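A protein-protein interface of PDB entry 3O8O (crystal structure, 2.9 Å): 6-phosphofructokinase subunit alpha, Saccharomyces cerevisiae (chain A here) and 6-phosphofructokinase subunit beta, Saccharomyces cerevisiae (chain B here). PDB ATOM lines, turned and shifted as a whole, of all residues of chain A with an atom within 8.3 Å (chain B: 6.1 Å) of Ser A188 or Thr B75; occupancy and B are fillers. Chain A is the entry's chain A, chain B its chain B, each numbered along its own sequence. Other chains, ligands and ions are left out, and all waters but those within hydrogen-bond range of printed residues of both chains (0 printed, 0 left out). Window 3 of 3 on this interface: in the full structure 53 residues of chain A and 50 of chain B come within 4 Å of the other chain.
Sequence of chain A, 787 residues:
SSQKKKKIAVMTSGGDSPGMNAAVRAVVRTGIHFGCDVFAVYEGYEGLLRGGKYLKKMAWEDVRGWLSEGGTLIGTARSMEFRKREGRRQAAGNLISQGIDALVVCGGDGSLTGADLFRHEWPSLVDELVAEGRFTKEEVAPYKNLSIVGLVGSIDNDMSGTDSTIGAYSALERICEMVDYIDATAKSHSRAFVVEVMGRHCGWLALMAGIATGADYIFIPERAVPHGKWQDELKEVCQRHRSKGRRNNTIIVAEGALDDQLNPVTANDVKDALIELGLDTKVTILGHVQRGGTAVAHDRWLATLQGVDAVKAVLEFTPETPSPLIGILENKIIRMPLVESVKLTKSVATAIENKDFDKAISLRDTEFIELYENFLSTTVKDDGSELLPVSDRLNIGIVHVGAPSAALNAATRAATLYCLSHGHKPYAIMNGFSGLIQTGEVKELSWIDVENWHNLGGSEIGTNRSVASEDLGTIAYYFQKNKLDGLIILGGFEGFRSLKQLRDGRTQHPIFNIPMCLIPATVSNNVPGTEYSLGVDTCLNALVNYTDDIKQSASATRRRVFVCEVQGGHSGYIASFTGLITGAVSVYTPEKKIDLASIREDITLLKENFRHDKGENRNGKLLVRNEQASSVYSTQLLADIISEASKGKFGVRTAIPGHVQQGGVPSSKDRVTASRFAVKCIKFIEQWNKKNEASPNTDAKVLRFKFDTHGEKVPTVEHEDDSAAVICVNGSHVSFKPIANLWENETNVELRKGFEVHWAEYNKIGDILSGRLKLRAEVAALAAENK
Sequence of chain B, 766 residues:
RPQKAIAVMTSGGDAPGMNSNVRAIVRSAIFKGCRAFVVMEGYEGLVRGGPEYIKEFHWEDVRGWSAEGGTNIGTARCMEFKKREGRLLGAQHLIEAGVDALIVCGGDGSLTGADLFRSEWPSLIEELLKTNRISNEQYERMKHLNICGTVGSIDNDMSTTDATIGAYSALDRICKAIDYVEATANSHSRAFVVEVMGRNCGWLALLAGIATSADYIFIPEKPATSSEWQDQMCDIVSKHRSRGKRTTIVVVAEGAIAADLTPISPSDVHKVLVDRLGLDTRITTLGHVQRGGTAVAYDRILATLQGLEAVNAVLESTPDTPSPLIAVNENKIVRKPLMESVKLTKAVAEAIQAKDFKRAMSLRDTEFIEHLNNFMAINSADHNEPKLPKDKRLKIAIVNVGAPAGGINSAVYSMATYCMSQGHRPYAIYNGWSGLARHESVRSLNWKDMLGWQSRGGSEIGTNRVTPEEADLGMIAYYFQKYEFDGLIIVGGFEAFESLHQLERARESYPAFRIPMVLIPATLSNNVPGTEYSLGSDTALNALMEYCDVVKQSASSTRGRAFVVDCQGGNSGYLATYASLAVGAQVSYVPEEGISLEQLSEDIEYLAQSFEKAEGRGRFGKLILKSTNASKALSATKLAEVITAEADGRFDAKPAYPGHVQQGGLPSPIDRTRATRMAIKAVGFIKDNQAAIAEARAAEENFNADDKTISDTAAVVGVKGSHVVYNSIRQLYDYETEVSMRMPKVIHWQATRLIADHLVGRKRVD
Of the 18 printed residues of chain B, 9 touch a printed residue of chain A.
Printed residues of chain B that touch a printed residue of chain A: Gly B12, Gly B13, Asp B14, Glu B41, Gly B69, Gly B70, Thr B71, Gly B74 and Thr B75.
Along chain B the printed residues that touch a printed residue of chain A span positions 12 to 75.
Hydrophobic or aromatic side chains of chain A within 4 Å of the printed part of chain B: Ala A184 and His A189.
Among the printed residues, pairs that only touch across the chains: Ser A188 with Gly B70 (3.2 Å), His A189 with Gly B12 (3.3 Å), His A189 with Gly B13 (3.7 Å), Ala A184 with Gly B69 (3.8 Å), Ala A184 with Gly B70 (3.8 Å), Ser A188 with Gly B74 (3.8 Å), Ala A184 with Asp B14 (3.96 Å) and Ser A190 with Glu B41 (3.998 Å).
The backbone carbonyl oxygen (O) of Thr B10 sits close to the side-chain hydroxyl (OG1) of Thr B75 (3.3 Å).
The backbone carbonyl oxygen of Ser A188 lies within hydrogen-bond range of the guanidinium group of Arg A247, at 3.4 Å.
The side-chain hydroxyl (OG) of Ser A190 lies within hydrogen-bond range of the guanidinium group (NH2) of Arg A247 (3.3 Å).
SD of Met B18 lies within hydrogen-bond range of OG1 of Thr B71.
The backbone carbonyl oxygen (O) of Ala A184 sits at hydrogen-bond distance from the side-chain hydroxyl (OG) of Ser A188 (3.3 Å).
The side-chain hydroxyl (OG1) of Thr B75 lies within hydrogen-bond range of the backbone carbonyl oxygen (O) of Gly B12, at 2.8 Å.
Of chain B, only Asp B14, Gly B70, Thr B71, Gly B74 and Thr B75 come within 4 Å of Ser A188.
Printed residues of chain B within 4 Å of His A189: Gly B12 (3.3 Å), Gly B13 (3.7 Å), Asp B14 (3.2 Å) and Thr B75 (3.2 Å).
Arg A191 touches none of the printed residues of chain B.
Gly B12 touches just one residue of chain A: His A189 (3.3 Å).
Of the printed residues of chain A, Asp B14 touches Ala A184 (3.96 Å), Thr A185 (2.8 Å), Ser A188 (3.0 Å) and His A189 (3.2 Å).
Of the printed residues of chain A, Gly B70 touches Ala A184 (3.8 Å) and Ser A188 (3.2 Å).
Ile B73 touches none of the printed residues of chain A.
Of the printed residues of chain A, Gly B74 touches Ser A188 (3.8 Å).
Thr B75 touches just these residues of chain A: Ser A188 and His A189.
No residue of chain A comes within 4 Å of Ala B76.
The nearest residue of chain A that does not touch Thr B75 is Arg A247 (5.0 Å).
OG of Ser A188 lies within hydrogen-bond range of OD2 of Asp B14 (3.0 Å).
The guanidinium group of Arg A247 is in salt-bridge range of the side-chain carboxylate of Glu B41 (2.9 Å).
The side-chain hydroxyl of Ser A188 is in hydrogen-bond range of the backbone NH of Thr B71 (2.8 Å).
The side-chain hydroxyl (OG1) of Thr A185 is in hydrogen-bond range of the side-chain carboxylate (OD1) of Asp B14, 2.8 Å away.
A ring nitrogen (ND1) of His A189 lies close to the backbone carbonyl oxygen (O) of Thr B75 (3.5 Å).
The backbone NH (N) of Thr B75 lies within hydrogen-bond range of the backbone carbonyl oxygen (O) of Ser A188, at 3.3 Å.
A ring nitrogen (NE2) of His A189 lies within hydrogen-bond range of the backbone NH (N) of Asp B14 (3.2 Å).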
ATOM      1  N   ILE A 182       0.775  -9.665 -13.099  1.00  0.00           N
ATOM      2  CA  ILE A 182       0.853 -10.293 -11.795  1.00  0.00           C
ATOM      3  C   ILE A 182       1.960  -9.676 -10.952  1.00  0.00           C
ATOM      4  O   ILE A 182       1.786  -9.455  -9.746  1.00  0.00           O
ATOM      5  CB  ILE A 182       1.103 -11.815 -11.933  1.00  0.00           C
ATOM      6  CG1 ILE A 182      -0.111 -12.482 -12.595  1.00  0.00           C
ATOM      7  CG2 ILE A 182       1.406 -12.429 -10.561  1.00  0.00           C
ATOM      8  CD1 ILE A 182       0.098 -13.956 -12.899  1.00  0.00           C
ATOM      9  N   ASP A 183       3.094  -9.394 -11.588  1.00  0.00           N
ATOM     10  CA  ASP A 183       4.222  -8.808 -10.880  1.00  0.00           C
ATOM     11  C   ASP A 183       3.826  -7.595 -10.069  1.00  0.00           C
ATOM     12  O   ASP A 183       4.171  -7.487  -8.892  1.00  0.00           O
ATOM     13  CB  ASP A 183       5.342  -8.427 -11.853  1.00  0.00           C
ATOM     14  CG  ASP A 183       6.243  -9.607 -12.199  1.00  0.00           C
ATOM     15  OD1 ASP A 183       7.084  -9.447 -13.120  1.00  0.00           O
ATOM     16  OD2 ASP A 183       6.115 -10.681 -11.551  1.00  0.00           O
ATOM     17  N   ALA A 184       3.078  -6.687 -10.672  1.00  0.00           N
ATOM     18  CA  ALA A 184       2.714  -5.491  -9.935  1.00  0.00           C
ATOM     19  C   ALA A 184       2.070  -5.798  -8.598  1.00  0.00           C
ATOM     20  O   ALA A 184       2.515  -5.319  -7.555  1.00  0.00           O
ATOM     21  CB  ALA A 184       1.808  -4.648 -10.747  1.00  0.00           C
ATOM     22  N   THR A 185       1.024  -6.606  -8.627  1.00  0.00           N
ATOM     23  CA  THR A 185       0.309  -6.940  -7.413  1.00  0.00           C
ATOM     24  C   THR A 185       1.139  -7.810  -6.485  1.00  0.00           C
ATOM     25  O   THR A 185       1.149  -7.582  -5.279  1.00  0.00           O
ATOM     26  CB  THR A 185      -1.026  -7.622  -7.748  1.00  0.00           C
ATOM     27  OG1 THR A 185      -1.799  -7.769  -6.550  1.00  0.00           O
ATOM     28  CG2 THR A 185      -0.786  -8.974  -8.403  1.00  0.00           C
ATOM     29  N   ALA A 186       1.844  -8.794  -7.036  1.00  0.00           N
ATOM     30  CA  ALA A 186       2.692  -9.661  -6.207  1.00  0.00           C
ATOM     31  C   ALA A 186       3.705  -8.824  -5.416  1.00  0.00           C
ATOM     32  O   ALA A 186       3.936  -9.063  -4.238  1.00  0.00           O
ATOM     33  CB  ALA A 186       3.425 -10.681  -7.081  1.00  0.00           C
ATOM     34  N   LYS A 187       4.304  -7.842  -6.081  1.00  0.00           N
ATOM     35  CA  LYS A 187       5.275  -6.956  -5.460  1.00  0.00           C
ATOM     36  C   LYS A 187       4.635  -6.206  -4.291  1.00  0.00           C
ATOM     37  O   LYS A 187       5.236  -6.077  -3.237  1.00  0.00           O
ATOM     38  N   SER A 188       3.417  -5.715  -4.477  1.00  0.00           N
ATOM     39  CA  SER A 188       2.719  -4.982  -3.425  1.00  0.00           C
ATOM     40  C   SER A 188       2.561  -5.762  -2.113  1.00  0.00           C
ATOM     41  O   SER A 188       2.790  -5.233  -1.012  1.00  0.00           O
ATOM     42  CB  SER A 188       1.313  -4.578  -3.891  1.00  0.00           C
ATOM     43  OG  SER A 188       1.326  -3.619  -4.926  1.00  0.00           O
ATOM     44  N   HIS A 189       2.141  -7.015  -2.238  1.00  0.00           N
ATOM     45  CA  HIS A 189       1.898  -7.863  -1.087  1.00  0.00           C
ATOM     46  C   HIS A 189       3.064  -8.804  -0.796  1.00  0.00           C
ATOM     47  O   HIS A 189       2.910  -9.788  -0.075  1.00  0.00           O
ATOM     48  CB  HIS A 189       0.610  -8.674  -1.314  1.00  0.00           C
ATOM     49  CG  HIS A 189      -0.627  -7.838  -1.481  1.00  0.00           C
ATOM     50  ND1 HIS A 189      -1.176  -7.099  -0.455  1.00  0.00           N
ATOM     51  CD2 HIS A 189      -1.429  -7.633  -2.554  1.00  0.00           C
ATOM     52  CE1 HIS A 189      -2.260  -6.477  -0.888  1.00  0.00           C
ATOM     53  NE2 HIS A 189      -2.437  -6.783  -2.159  1.00  0.00           N
ATOM     54  N   SER A 190       4.226  -8.510  -1.356  1.00  0.00           N
ATOM     55  CA  SER A 190       5.416  -9.342  -1.145  1.00  0.00           C
ATOM     56  C   SER A 190       5.089 -10.832  -1.164  1.00  0.00           C
ATOM     57  O   SER A 190       5.636 -11.604  -0.382  1.00  0.00           O
ATOM     58  CB  SER A 190       6.079  -9.001   0.197  1.00  0.00           C
ATOM     59  OG  SER A 190       6.220  -7.602   0.381  1.00  0.00           O
ATOM     60  N   ARG A 191       4.209 -11.234  -2.070  1.00  0.00           N
ATOM     61  CA  ARG A 191       3.798 -12.627  -2.179  1.00  0.00           C
ATOM     62  C   ARG A 191       4.641 -13.494  -3.079  1.00  0.00           C
ATOM     63  O   ARG A 191       5.708 -13.114  -3.535  1.00  0.00           O
ATOM     64  CB  ARG A 191       2.380 -12.693  -2.692  1.00  0.00           C
ATOM     65  CG  ARG A 191       1.425 -12.032  -1.783  1.00  0.00           C
ATOM     66  CD  ARG A 191       0.071 -11.981  -2.400  1.00  0.00           C
ATOM     67  NE  ARG A 191      -0.923 -11.758  -1.369  1.00  0.00           N
ATOM     68  CZ  ARG A 191      -2.183 -11.459  -1.623  1.00  0.00           C
ATOM     69  NH1 ARG A 191      -2.588 -11.347  -2.876  1.00  0.00           N
ATOM     70  NH2 ARG A 191      -3.034 -11.279  -0.630  1.00  0.00           N
ATOM     71  N   PHE A 193       3.860 -16.109  -6.381  1.00  0.00           N
ATOM     72  CA  PHE A 193       2.847 -16.692  -7.247  1.00  0.00           C
ATOM     73  C   PHE A 193       3.356 -17.872  -8.026  1.00  0.00           C
ATOM     74  O   PHE A 193       4.484 -17.881  -8.531  1.00  0.00           O
ATOM     75  CB  PHE A 193       2.308 -15.700  -8.233  1.00  0.00           C
ATOM     76  CG  PHE A 193       1.263 -14.828  -7.684  1.00  0.00           C
ATOM     77  CD1 PHE A 193       1.564 -13.915  -6.674  1.00  0.00           C
ATOM     78  CD2 PHE A 193      -0.012 -14.827  -8.265  1.00  0.00           C
ATOM     79  CE1 PHE A 193       0.600 -12.972  -6.244  1.00  0.00           C
ATOM     80  CE2 PHE A 193      -0.999 -13.898  -7.860  1.00  0.00           C
ATOM     81  CZ  PHE A 193      -0.687 -12.956  -6.839  1.00  0.00           C
ATOM     82  N   ARG A 247      11.010  -9.124  -2.986  1.00  0.00           N
ATOM     83  CA  ARG A 247       9.748  -9.080  -2.263  1.00  0.00           C
ATOM     84  C   ARG A 247       8.783 -10.171  -2.660  1.00  0.00           C
ATOM     85  O   ARG A 247       8.054 -10.699  -1.826  1.00  0.00           O
ATOM     86  CB  ARG A 247       9.035  -7.757  -2.492  1.00  0.00           C
ATOM     87  CG  ARG A 247       9.761  -6.573  -1.962  1.00  0.00           C
ATOM     88  CD  ARG A 247       9.155  -5.336  -2.521  1.00  0.00           C
ATOM     89  NE  ARG A 247       7.783  -5.216  -2.095  1.00  0.00           N
ATOM     90  CZ  ARG A 247       7.424  -4.569  -0.999  1.00  0.00           C
ATOM     91  NH1 ARG A 247       8.350  -3.992  -0.240  1.00  0.00           N
ATOM     92  NH2 ARG A 247       6.143  -4.510  -0.661  1.00  0.00           N
ATOM     93  N   ASN A 248       8.748 -10.493  -3.942  1.00  0.00           N
ATOM     94  CA  ASN A 248       7.824 -11.501  -4.430  1.00  0.00           C
ATOM     95  C   ASN A 248       8.557 -12.593  -5.178  1.00  0.00           C
ATOM     96  O   ASN A 248       9.581 -12.334  -5.810  1.00  0.00           O
ATOM     97  CB  ASN A 248       6.830 -10.845  -5.371  1.00  0.00           C
ATOM     98  CG  ASN A 248       7.495 -10.319  -6.609  1.00  0.00           C
ATOM     99  OD1 ASN A 248       7.345 -10.878  -7.695  1.00  0.00           O
ATOM    100  ND2 ASN A 248       8.263  -9.253  -6.452  1.00  0.00           N
ATOM    101  N   ASP A 280       2.992 -15.953   1.735  1.00  0.00           N
ATOM    102  CA  ASP A 280       1.629 -15.720   1.269  1.00  0.00           C
ATOM    103  C   ASP A 280       1.665 -16.205  -0.174  1.00  0.00           C
ATOM    104  O   ASP A 280       2.285 -15.554  -1.014  1.00  0.00           O
ATOM    105  CB  ASP A 280       1.330 -14.229   1.285  1.00  0.00           C
ATOM    106  CG  ASP A 280      -0.149 -13.922   1.097  1.00  0.00           C
ATOM    107  OD1 ASP A 280      -0.881 -14.774   0.533  1.00  0.00           O
ATOM    108  OD2 ASP A 280      -0.574 -12.814   1.511  1.00  0.00           O
ATOM    109  N   THR B  10      -1.071   2.771   1.891  1.00  0.00           N
ATOM    110  CA  THR B  10      -2.018   2.012   1.088  1.00  0.00           C
ATOM    111  C   THR B  10      -2.275   0.744   1.862  1.00  0.00           C
ATOM    112  O   THR B  10      -1.350   0.000   2.168  1.00  0.00           O
ATOM    113  CB  THR B  10      -1.475   1.614  -0.302  1.00  0.00           C
ATOM    114  OG1 THR B  10      -0.287   0.819  -0.151  1.00  0.00           O
ATOM    115  CG2 THR B  10      -1.224   2.851  -1.154  1.00  0.00           C
ATOM    116  N   SER B  11      -3.533   0.495   2.181  1.00  0.00           N
ATOM    117  CA  SER B  11      -3.856  -0.686   2.945  1.00  0.00           C
ATOM    118  C   SER B  11      -4.854  -1.519   2.188  1.00  0.00           C
ATOM    119  O   SER B  11      -5.602  -0.998   1.354  1.00  0.00           O
ATOM    120  CB  SER B  11      -4.436  -0.277   4.296  1.00  0.00           C
ATOM    121  OG  SER B  11      -4.612  -1.407   5.122  1.00  0.00           O
ATOM    122  N   GLY B  12      -4.864  -2.816   2.476  1.00  0.00           N
ATOM    123  CA  GLY B  12      -5.805  -3.697   1.815  1.00  0.00           C
ATOM    124  C   GLY B  12      -5.273  -4.139   0.476  1.00  0.00           C
ATOM    125  O   GLY B  12      -4.098  -3.912   0.165  1.00  0.00           O
ATOM    126  N   GLY B  13      -6.140  -4.761  -0.319  1.00  0.00           N
ATOM    127  CA  GLY B  13      -5.739  -5.253  -1.626  1.00  0.00           C
ATOM    128  C   GLY B  13      -5.340  -4.105  -2.501  1.00  0.00           C
ATOM    129  O   GLY B  13      -6.090  -3.144  -2.628  1.00  0.00           O
ATOM    130  N   ASP B  14      -4.155  -4.207  -3.091  1.00  0.00           N
ATOM    131  CA  ASP B  14      -3.638  -3.154  -3.965  1.00  0.00           C
ATOM    132  C   ASP B  14      -4.528  -3.086  -5.194  1.00  0.00           C
ATOM    133  O   ASP B  14      -5.206  -4.058  -5.534  1.00  0.00           O
ATOM    134  CB  ASP B  14      -2.177  -3.455  -4.379  1.00  0.00           C
ATOM    135  CG  ASP B  14      -2.052  -4.688  -5.294  1.00  0.00           C
ATOM    136  OD1 ASP B  14      -2.858  -5.635  -5.160  1.00  0.00           O
ATOM    137  OD2 ASP B  14      -1.137  -4.717  -6.139  1.00  0.00           O
ATOM    138  N   MET B  18      -3.010   3.213  -7.357  1.00  0.00           N
ATOM    139  CA  MET B  18      -2.639   3.676  -6.031  1.00  0.00           C
ATOM    140  C   MET B  18      -1.404   4.557  -6.138  1.00  0.00           C
ATOM    141  O   MET B  18      -1.306   5.580  -5.451  1.00  0.00           O
ATOM    142  CB  MET B  18      -2.371   2.498  -5.098  1.00  0.00           C
ATOM    143  CG  MET B  18      -3.594   1.639  -4.877  1.00  0.00           C
ATOM    144  SD  MET B  18      -3.436   0.428  -3.547  1.00  0.00           S
ATOM    145  CE  MET B  18      -4.827   0.867  -2.590  1.00  0.00           C
ATOM    146  N   MET B  40       5.382   2.818   4.802  1.00  0.00           N
ATOM    147  CA  MET B  40       5.623   1.542   4.150  1.00  0.00           C
ATOM    148  C   MET B  40       4.792   0.396   4.742  1.00  0.00           C
ATOM    149  O   MET B  40       4.395   0.439   5.902  1.00  0.00           O
ATOM    150  CB  MET B  40       7.112   1.205   4.227  1.00  0.00           C
ATOM    151  CG  MET B  40       8.004   2.274   3.609  1.00  0.00           C
ATOM    152  SD  MET B  40       7.721   2.554   1.850  1.00  0.00           S
ATOM    153  CE  MET B  40       9.401   2.581   1.263  1.00  0.00           C
ATOM    154  N   GLU B  41       4.523  -0.613   3.918  1.00  0.00           N
ATOM    155  CA  GLU B  41       3.770  -1.798   4.307  1.00  0.00           C
ATOM    156  C   GLU B  41       2.482  -1.605   5.102  1.00  0.00           C
ATOM    157  O   GLU B  41       2.232  -2.350   6.051  1.00  0.00           O
ATOM    158  CB  GLU B  41       4.677  -2.752   5.075  1.00  0.00           C
ATOM    159  CG  GLU B  41       5.878  -3.228   4.285  1.00  0.00           C
ATOM    160  CD  GLU B  41       5.508  -3.862   2.964  1.00  0.00           C
ATOM    161  OE1 GLU B  41       4.803  -4.898   2.962  1.00  0.00           O
ATOM    162  OE2 GLU B  41       5.929  -3.313   1.924  1.00  0.00           O
ATOM    163  N   GLY B  42       1.666  -0.622   4.721  1.00  0.00           N
ATOM    164  CA  GLY B  42       0.399  -0.392   5.408  1.00  0.00           C
ATOM    165  C   GLY B  42       0.466  -0.091   6.897  1.00  0.00           C
ATOM    166  O   GLY B  42       1.417   0.528   7.366  1.00  0.00           O
ATOM    167  N   GLY B  69       2.475  -0.165 -11.715  1.00  0.00           N
ATOM    168  CA  GLY B  69       1.440  -0.925 -11.040  1.00  0.00           C
ATOM    169  C   GLY B  69       1.615  -1.100  -9.539  1.00  0.00           C
ATOM    170  O   GLY B  69       2.660  -0.789  -8.978  1.00  0.00           O
ATOM    171  N   GLY B  70       0.569  -1.609  -8.893  1.00  0.00           N
ATOM    172  CA  GLY B  70       0.591  -1.834  -7.457  1.00  0.00           C
ATOM    173  C   GLY B  70       0.865  -0.595  -6.626  1.00  0.00           C
ATOM    174  O   GLY B  70       0.608   0.535  -7.046  1.00  0.00           O
ATOM    175  N   THR B  71       1.374  -0.827  -5.423  1.00  0.00           N
ATOM    176  CA  THR B  71       1.733   0.237  -4.500  1.00  0.00           C
ATOM    177  C   THR B  71       3.225   0.201  -4.338  1.00  0.00           C
ATOM    178  O   THR B  71       3.771  -0.812  -3.879  1.00  0.00           O
ATOM    179  CB  THR B  71       1.241   0.017  -3.078  1.00  0.00           C
ATOM    180  OG1 THR B  71      -0.167  -0.183  -3.071  1.00  0.00           O
ATOM    181  CG2 THR B  71       1.571   1.224  -2.238  1.00  0.00           C
ATOM    182  N   ASN B  72       3.898   1.295  -4.677  1.00  0.00           N
ATOM    183  CA  ASN B  72       5.331   1.311  -4.487  1.00  0.00           C
ATOM    184  C   ASN B  72       5.664   1.364  -2.987  1.00  0.00           C
ATOM    185  O   ASN B  72       6.739   0.922  -2.566  1.00  0.00           O
ATOM    186  CB  ASN B  72       5.960   2.469  -5.252  1.00  0.00           C
ATOM    187  CG  ASN B  72       5.951   2.236  -6.744  1.00  0.00           C
ATOM    188  OD1 ASN B  72       5.755   1.112  -7.200  1.00  0.00           O
ATOM    189  ND2 ASN B  72       6.171   3.290  -7.514  1.00  0.00           N
ATOM    190  N   ILE B  73       4.738   1.865  -2.172  1.00  0.00           N
ATOM    191  CA  ILE B  73       4.990   1.911  -0.733  1.00  0.00           C
ATOM    192  C   ILE B  73       4.479   0.632  -0.038  1.00  0.00           C
ATOM    193  O   ILE B  73       4.585   0.481   1.185  1.00  0.00           O
ATOM    194  CB  ILE B  73       4.373   3.191  -0.093  1.00  0.00           C
ATOM    195  CG1 ILE B  73       2.823   3.112  -0.062  1.00  0.00           C
ATOM    196  CG2 ILE B  73       4.861   4.393  -0.876  1.00  0.00           C
ATOM    197  CD1 ILE B  73       2.126   4.396   0.367  1.00  0.00           C
ATOM    198  N   GLY B  74       3.939  -0.291  -0.835  1.00  0.00           N
ATOM    199  CA  GLY B  74       3.446  -1.559  -0.308  1.00  0.00           C
ATOM    200  C   GLY B  74       2.183  -1.557   0.545  1.00  0.00           C
ATOM    201  O   GLY B  74       1.602  -0.504   0.854  1.00  0.00           O
ATOM    202  N   THR B  75       1.752  -2.760   0.921  1.00  0.00           N
ATOM    203  CA  THR B  75       0.566  -2.944   1.759  1.00  0.00           C
ATOM    204  C   THR B  75       0.681  -4.327   2.362  1.00  0.00           C
ATOM    205  O   THR B  75       0.953  -5.299   1.654  1.00  0.00           O
ATOM    206  CB  THR B  75      -0.731  -2.848   0.935  1.00  0.00           C
ATOM    207  OG1 THR B  75      -1.859  -3.219   1.741  1.00  0.00           O
ATOM    208  CG2 THR B  75      -0.637  -3.757  -0.279  1.00  0.00           C
ATOM    209  N   ALA B  76       0.508  -4.409   3.680  1.00  0.00           N
ATOM    210  CA  ALA B  76       0.603  -5.687   4.386  1.00  0.00           C
ATOM    211  C   ALA B  76      -0.630  -5.959   5.239  1.00  0.00           C
ATOM    212  O   ALA B  76      -1.434  -5.060   5.502  1.00  0.00           O
ATOM    213  CB  ALA B  76       1.854  -5.718   5.252  1.00  0.00           C
ATOM    214  N   ARG B  77      -0.779  -7.217   5.646  1.00  0.00           N
ATOM    215  CA  ARG B  77      -1.906  -7.633   6.465  1.00  0.00           C
ATOM    216  C   ARG B  77      -1.565  -7.124   7.854  1.00  0.00           C
ATOM    217  O   ARG B  77      -0.462  -7.365   8.360  1.00  0.00           O
